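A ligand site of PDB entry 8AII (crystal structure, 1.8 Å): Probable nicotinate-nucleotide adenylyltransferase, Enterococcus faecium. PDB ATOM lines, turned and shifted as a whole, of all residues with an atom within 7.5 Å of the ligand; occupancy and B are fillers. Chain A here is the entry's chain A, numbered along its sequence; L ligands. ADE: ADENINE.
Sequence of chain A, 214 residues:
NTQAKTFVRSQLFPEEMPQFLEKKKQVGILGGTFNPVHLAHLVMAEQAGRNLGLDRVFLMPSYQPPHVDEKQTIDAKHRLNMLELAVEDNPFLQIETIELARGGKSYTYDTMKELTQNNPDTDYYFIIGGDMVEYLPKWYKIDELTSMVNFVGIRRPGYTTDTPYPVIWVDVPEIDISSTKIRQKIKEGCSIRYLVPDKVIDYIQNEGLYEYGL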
ATOM      1  N   GLY A  31      17.513  17.628   1.975  1.00  0.00           N
ATOM      2  CA  GLY A  31      16.645  16.466   1.981  1.00  0.00           C
ATOM      3  C   GLY A  31      15.385  16.705   2.810  1.00  0.00           C
ATOM      4  O   GLY A  31      15.320  17.647   3.594  1.00  0.00           O
ATOM      5  N   GLY A  32      14.399  15.859   2.584  1.00  0.00           N
ATOM      6  CA  GLY A  32      13.111  15.979   3.255  1.00  0.00           C
ATOM      7  C   GLY A  32      12.098  15.097   2.564  1.00  0.00           C
ATOM      8  O   GLY A  32      12.332  14.585   1.473  1.00  0.00           O
ATOM      9  N   THR A  33      10.958  14.922   3.216  1.00  0.00           N
ATOM     10  CA  THR A  33       9.823  14.284   2.560  1.00  0.00           C
ATOM     11  C   THR A  33       9.129  15.222   1.582  1.00  0.00           C
ATOM     12  O   THR A  33       8.623  14.767   0.549  1.00  0.00           O
ATOM     13  CB  THR A  33       8.796  13.791   3.582  1.00  0.00           C
ATOM     14  OG1 THR A  33       8.335  14.897   4.362  1.00  0.00           O
ATOM     15  CG2 THR A  33       9.401  12.747   4.499  1.00  0.00           C
ATOM     16  N   PHE A  34       9.092  16.515   1.901  1.00  0.00           N
ATOM     17  CA  PHE A  34       8.397  17.539   1.128  1.00  0.00           C
ATOM     18  C   PHE A  34       6.952  17.116   0.851  1.00  0.00           C
ATOM     19  O   PHE A  34       6.535  16.911  -0.289  1.00  0.00           O
ATOM     20  CB  PHE A  34       9.137  17.864  -0.156  1.00  0.00           C
ATOM     21  CG  PHE A  34      10.583  18.248   0.061  1.00  0.00           C
ATOM     22  CD1 PHE A  34      10.940  19.515   0.471  1.00  0.00           C
ATOM     23  CD2 PHE A  34      11.592  17.327  -0.166  1.00  0.00           C
ATOM     24  CE1 PHE A  34      12.290  19.866   0.651  1.00  0.00           C
ATOM     25  CE2 PHE A  34      12.942  17.662   0.022  1.00  0.00           C
ATOM     26  CZ  PHE A  34      13.290  18.919   0.413  1.00  0.00           C
ATOM     27  N   ASN A  35       6.194  16.986   1.928  1.00  0.00           N
ATOM     28  CA  ASN A  35       4.845  16.406   1.882  1.00  0.00           C
ATOM     29  C   ASN A  35       3.858  17.311   2.609  1.00  0.00           C
ATOM     30  O   ASN A  35       3.231  16.903   3.589  1.00  0.00           O
ATOM     31  CB  ASN A  35       4.875  15.004   2.483  1.00  0.00           C
ATOM     32  CG  ASN A  35       3.578  14.275   2.324  1.00  0.00           C
ATOM     33  OD1 ASN A  35       2.844  14.480   1.350  1.00  0.00           O
ATOM     34  ND2 ASN A  35       3.271  13.404   3.266  1.00  0.00           N
ATOM     35  N   PRO A  36       3.645  18.543   2.105  1.00  0.00           N
ATOM     36  CA  PRO A  36       4.143  19.126   0.854  1.00  0.00           C
ATOM     37  C   PRO A  36       5.317  20.078   1.035  1.00  0.00           C
ATOM     38  O   PRO A  36       5.591  20.521   2.153  1.00  0.00           O
ATOM     39  CB  PRO A  36       2.928  19.904   0.371  1.00  0.00           C
ATOM     40  CG  PRO A  36       2.390  20.478   1.666  1.00  0.00           C
ATOM     41  CD  PRO A  36       2.673  19.437   2.751  1.00  0.00           C
ATOM     42  N   VAL A  37       5.985  20.405  -0.066  1.00  0.00           N
ATOM     43  CA  VAL A  37       6.969  21.497  -0.088  1.00  0.00           C
ATOM     44  C   VAL A  37       6.318  22.769   0.449  1.00  0.00           C
ATOM     45  O   VAL A  37       5.115  22.981   0.277  1.00  0.00           O
ATOM     46  CB  VAL A  37       7.503  21.700  -1.516  1.00  0.00           C
ATOM     47  CG1 VAL A  37       6.380  22.144  -2.453  1.00  0.00           C
ATOM     48  CG2 VAL A  37       8.678  22.669  -1.555  1.00  0.00           C
ATOM     49  N   HIS A  38       7.093  23.644   1.099  1.00  0.00           N
ATOM     50  CA  HIS A  38       6.527  24.872   1.665  1.00  0.00           C
ATOM     51  C   HIS A  38       7.606  25.945   1.790  1.00  0.00           C
ATOM     52  O   HIS A  38       8.761  25.728   1.444  1.00  0.00           O
ATOM     53  CB  HIS A  38       5.893  24.618   3.032  1.00  0.00           C
ATOM     54  CG  HIS A  38       6.812  23.941   4.000  1.00  0.00           C
ATOM     55  ND1 HIS A  38       7.960  24.534   4.463  1.00  0.00           N
ATOM     56  CD2 HIS A  38       6.754  22.708   4.560  1.00  0.00           C
ATOM     57  CE1 HIS A  38       8.572  23.701   5.282  1.00  0.00           C
ATOM     58  NE2 HIS A  38       7.870  22.590   5.359  1.00  0.00           N
ATOM     59  N   ALA A  40       9.380  27.309   4.083  1.00  0.00           N
ATOM     60  CA  ALA A  40      10.616  27.144   4.836  1.00  0.00           C
ATOM     61  C   ALA A  40      11.654  26.357   4.036  1.00  0.00           C
ATOM     62  O   ALA A  40      12.846  26.661   4.079  1.00  0.00           O
ATOM     63  CB  ALA A  40      10.347  26.472   6.179  1.00  0.00           C
ATOM     64  N   HIS A  41      11.198  25.353   3.263  1.00  0.00           N
ATOM     65  CA  HIS A  41      12.116  24.638   2.364  1.00  0.00           C
ATOM     66  C   HIS A  41      12.803  25.598   1.408  1.00  0.00           C
ATOM     67  O   HIS A  41      14.016  25.516   1.193  1.00  0.00           O
ATOM     68  CB  HIS A  41      11.363  23.589   1.553  1.00  0.00           C
ATOM     69  CG  HIS A  41      10.764  22.490   2.363  1.00  0.00           C
ATOM     70  ND1 HIS A  41       9.445  22.113   2.243  1.00  0.00           N
ATOM     71  CD2 HIS A  41      11.314  21.655   3.287  1.00  0.00           C
ATOM     72  CE1 HIS A  41       9.205  21.099   3.046  1.00  0.00           C
ATOM     73  NE2 HIS A  41      10.315  20.819   3.704  1.00  0.00           N
ATOM     74  N   MET A  44      15.221  28.043   3.331  1.00  0.00           N
ATOM     75  CA  MET A  44      16.411  27.336   3.812  1.00  0.00           C
ATOM     76  C   MET A  44      17.364  27.034   2.669  1.00  0.00           C
ATOM     77  O   MET A  44      18.575  27.271   2.759  1.00  0.00           O
ATOM     78  CB  MET A  44      16.011  26.061   4.530  1.00  0.00           C
ATOM     79  CG  MET A  44      15.503  26.232   5.944  1.00  0.00           C
ATOM     80  SD  MET A  44      15.293  24.641   6.775  1.00  0.00           S
ATOM     81  CE  MET A  44      14.038  23.863   5.754  1.00  0.00           C
ATOM     82  N   SER A  62      12.731  12.355  -0.279  1.00  0.00           N
ATOM     83  CA  SER A  62      13.023  10.989   0.115  1.00  0.00           C
ATOM     84  C   SER A  62      11.925  10.054  -0.396  1.00  0.00           C
ATOM     85  O   SER A  62      10.850  10.489  -0.809  1.00  0.00           O
ATOM     86  CB  SER A  62      13.156  10.902   1.632  1.00  0.00           C
ATOM     87  OG  SER A  62      11.914  11.190   2.250  1.00  0.00           O
ATOM     88  N   ARG A  79       4.101  14.777  -4.858  1.00  0.00           N
ATOM     89  CA  ARG A  79       5.180  15.485  -4.184  1.00  0.00           C
ATOM     90  C   ARG A  79       6.144  16.093  -5.189  1.00  0.00           C
ATOM     91  O   ARG A  79       6.620  17.221  -5.009  1.00  0.00           O
ATOM     92  CB  ARG A  79       5.920  14.540  -3.243  1.00  0.00           C
ATOM     93  CG  ARG A  79       5.113  14.069  -2.044  1.00  0.00           C
ATOM     94  CD  ARG A  79       6.021  13.454  -0.989  1.00  0.00           C
ATOM     95  NE  ARG A  79       6.477  12.120  -1.377  1.00  0.00           N
ATOM     96  CZ  ARG A  79       7.709  11.653  -1.191  1.00  0.00           C
ATOM     97  NH1 ARG A  79       8.662  12.406  -0.618  1.00  0.00           N
ATOM     98  NH2 ARG A  79       8.004  10.423  -1.595  1.00  0.00           N
ATOM     99  N   ASP A 131      18.371  21.431  14.384  1.00  0.00           N
ATOM    100  CA  ASP A 131      17.782  20.405  15.245  1.00  0.00           C
ATOM    101  C   ASP A 131      18.246  19.005  14.855  1.00  0.00           C
ATOM    102  O   ASP A 131      18.389  18.137  15.726  1.00  0.00           O
ATOM    103  CB  ASP A 131      16.261  20.513  15.203  1.00  0.00           C
ATOM    104  CG  ASP A 131      15.729  20.771  13.800  1.00  0.00           C
ATOM    105  OD1 ASP A 131      16.414  21.441  13.002  1.00  0.00           O
ATOM    106  OD2 ASP A 131      14.606  20.319  13.500  1.00  0.00           O
ATOM    107  N   MET A 132      18.543  18.761  13.594  1.00  0.00           N
ATOM    108  CA  MET A 132      18.874  17.380  13.165  1.00  0.00           C
ATOM    109  C   MET A 132      20.333  17.048  13.458  1.00  0.00           C
ATOM    110  O   MET A 132      20.660  15.874  13.541  1.00  0.00           O
ATOM    111  CB  MET A 132      18.597  17.184  11.683  1.00  0.00           C
ATOM    112  CG  MET A 132      17.341  17.857  11.186  1.00  0.00           C
ATOM    113  SD  MET A 132      17.288  17.898   9.382  1.00  0.00           S
ATOM    114  CE  MET A 132      17.643  16.178   9.020  1.00  0.00           C
ATOM    115  N   ILE A 175      12.137  30.030  10.105  1.00  0.00           N
ATOM    116  CA  ILE A 175      10.810  29.875   9.513  1.00  0.00           C
ATOM    117  C   ILE A 175      10.216  28.604  10.093  1.00  0.00           C
ATOM    118  O   ILE A 175      10.573  27.493   9.666  1.00  0.00           O
ATOM    119  CB  ILE A 175      10.866  29.789   7.983  1.00  0.00           C
ATOM    120  CG1 ILE A 175      11.855  30.786   7.402  1.00  0.00           C
ATOM    121  CG2 ILE A 175       9.475  29.982   7.402  1.00  0.00           C
ATOM    122  CD1 ILE A 175      11.451  32.196   7.593  1.00  0.00           C
ATOM    123  N   ILE A 177       7.794  26.473   9.974  1.00  0.00           N
ATOM    124  CA  ILE A 177       6.796  25.770   9.179  1.00  0.00           C
ATOM    125  C   ILE A 177       7.289  24.338   8.998  1.00  0.00           C
ATOM    126  O   ILE A 177       8.492  24.120   8.807  1.00  0.00           O
ATOM    127  CB  ILE A 177       6.583  26.433   7.799  1.00  0.00           C
ATOM    128  CG1 ILE A 177       6.155  27.897   7.932  1.00  0.00           C
ATOM    129  CG2 ILE A 177       5.590  25.632   6.945  1.00  0.00           C
ATOM    130  CD1 ILE A 177       6.155  28.617   6.578  1.00  0.00           C
ATOM    131  N   SER A 178       6.385  23.372   9.045  1.00  0.00           N
ATOM    132  CA  SER A 178       6.721  21.996   8.711  1.00  0.00           C
ATOM    133  C   SER A 178       5.606  21.381   7.883  1.00  0.00           C
ATOM    134  O   SER A 178       4.442  21.763   8.023  1.00  0.00           O
ATOM    135  CB  SER A 178       6.961  21.141   9.957  1.00  0.00           C
ATOM    136  OG  SER A 178       5.732  20.836  10.585  1.00  0.00           O
ATOM    137  N   SER A 179       5.973  20.426   7.031  1.00  0.00           N
ATOM    138  CA  SER A 179       4.971  19.740   6.218  1.00  0.00           C
ATOM    139  C   SER A 179       3.842  19.218   7.078  1.00  0.00           C
ATOM    140  O   SER A 179       2.662  19.380   6.742  1.00  0.00           O
ATOM    141  CB  SER A 179       5.632  18.610   5.434  1.00  0.00           C
ATOM    142  OG  SER A 179       6.358  19.147   4.358  1.00  0.00           O
ATOM    143  N   THR A 180       4.171  18.614   8.216  1.00  0.00           N
ATOM    144  CA  THR A 180       3.121  18.136   9.121  1.00  0.00           C
ATOM    145  C   THR A 180       2.177  19.253   9.527  1.00  0.00           C
ATOM    146  O   THR A 180       0.948  19.071   9.526  1.00  0.00           O
ATOM    147  CB  THR A 180       3.756  17.468  10.341  1.00  0.00           C
ATOM    148  OG1 THR A 180       4.511  16.316   9.917  1.00  0.00           O
ATOM    149  CG2 THR A 180       2.712  17.062  11.329  1.00  0.00           C
ATOM    150  N   LYS A 181       2.729  20.430   9.871  1.00  0.00           N
ATOM    151  CA  LYS A 181       1.898  21.574  10.255  1.00  0.00           C
ATOM    152  C   LYS A 181       0.923  21.919   9.126  1.00  0.00           C
ATOM    153  O   LYS A 181      -0.276  22.076   9.360  1.00  0.00           O
ATOM    154  CB  LYS A 181       2.789  22.769  10.577  1.00  0.00           C
ATOM    155  CG  LYS A 181       2.729  23.294  11.996  1.00  0.00           C
ATOM    156  CD  LYS A 181       3.635  24.521  12.148  1.00  0.00           C
ATOM    157  CE  LYS A 181       3.560  25.117  13.551  1.00  0.00           C
ATOM    158  NZ  LYS A 181       4.283  26.425  13.679  1.00  0.00           N
ATOM    159  N   ILE A 182       1.445  22.043   7.903  1.00  0.00           N
ATOM    160  CA  ILE A 182       0.622  22.392   6.747  1.00  0.00           C
ATOM    161  C   ILE A 182      -0.488  21.361   6.554  1.00  0.00           C
ATOM    162  O   ILE A 182      -1.672  21.714   6.462  1.00  0.00           O
ATOM    163  CB  ILE A 182       1.509  22.513   5.500  1.00  0.00           C
ATOM    164  CG1 ILE A 182       2.456  23.725   5.625  1.00  0.00           C
ATOM    165  CG2 ILE A 182       0.666  22.579   4.211  1.00  0.00           C
ATOM    166  CD1 ILE A 182       1.725  25.037   5.982  1.00  0.00           C
ATOM    167  N   ARG A 183      -0.121  20.064   6.499  1.00  0.00           N
ATOM    168  CA  ARG A 183      -1.140  19.014   6.379  1.00  0.00           C
ATOM    169  C   ARG A 183      -2.187  19.131   7.471  1.00  0.00           C
ATOM    170  O   ARG A 183      -3.390  18.972   7.210  1.00  0.00           O
ATOM    171  CB  ARG A 183      -0.509  17.619   6.435  1.00  0.00           C
ATOM    172  CG  ARG A 183       0.318  17.257   5.207  1.00  0.00           C
ATOM    173  CD  ARG A 183       0.558  15.735   5.158  1.00  0.00           C
ATOM    174  NE  ARG A 183       0.984  15.198   6.445  1.00  0.00           N
ATOM    175  CZ  ARG A 183       2.248  15.255   6.894  1.00  0.00           C
ATOM    176  NH1 ARG A 183       3.187  15.826   6.157  1.00  0.00           N
ATOM    177  NH2 ARG A 183       2.559  14.747   8.074  1.00  0.00           N
HETATM  178  N9  ADE L   1       8.958  20.176   6.628  1.00  0.00           N
HETATM  179  C8  ADE L   1       9.523  20.343   7.820  1.00  0.00           C
HETATM  180  N7  ADE L   1      10.426  19.384   8.005  1.00  0.00           N
HETATM  181  C5  ADE L   1      10.431  18.591   6.902  1.00  0.00           C
HETATM  182  C6  ADE L   1      11.173  17.431   6.513  1.00  0.00           C
HETATM  183  N6  ADE L   1      12.184  16.858   7.381  1.00  0.00           N
HETATM  184  N1  ADE L   1      10.931  16.890   5.348  1.00  0.00           N
HETATM  185  C2  ADE L   1      10.026  17.418   4.545  1.00  0.00           C
HETATM  186  N3  ADE L   1       9.317  18.467   4.853  1.00  0.00           N
HETATM  187  C4  ADE L   1       9.509  19.091   6.047  1.00  0.00           C
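The backbone NH (N) of Thr 33 sits at hydrogen-bond distance from a nitrogen (N1) of the ligand.
N1 of the ligand sits close to OG1 of Thr 33.
NE2 of His 41 is in hydrogen-bond range of N3 of the ligand.
N9 of the ligand sits at hydrogen-bond distance from NE2 of His 38, 2.9 Å away.
The backbone NH of Ser 179 lies close to a nitrogen (N9) of the ligand (3.0 Å).
OG of Ser 179 is in hydrogen-bond range of N3 of the ligand (3.1 Å).
NE2 of His 38 is in hydrogen-bond range of N of Ser 179, at 3.3 Å.
O of Pro 36 sits at hydrogen-bond distance from OG of Ser 179.
OG of Ser 179 sits at hydrogen-bond distance from N of Asn 35 (3.3 Å).
The backbone carbonyl oxygen (O) of Gly 32 sits at hydrogen-bond distance from the backbone NH (N) of Ser 62.
The side-chain hydroxyl (OG) of Ser 178 is in hydrogen-bond range of the backbone NH (N) of Lys 181.
A ring nitrogen (ND1) of His 41 lies within hydrogen-bond range of the backbone NH of His 38, 3.0 Å away.
The backbone carbonyl oxygen of Thr 33 sits at hydrogen-bond distance from the guanidinium group of Arg 79 (2.6 Å).
A ring nitrogen (ND1) of His 38 lies within hydrogen-bond range of the backbone NH (N) of Ala 40 (3.1 Å).
CA of Gly 32 touches N1 of the ligand (3.2 Å).
Phe 34 touches the ligand (N to C2, 2.9 Å).
Ser 178 touches the ligand (CA to C8, 3.4 Å).
Hydrophobic or aromatic side chains that line the ligand: His 38 and His 41.
Of the 23 residues printed, 7 come within 4 Å of the ligand.
The nearest printed residue that does not touch the ligand is Ile 177 (4.04 Å).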
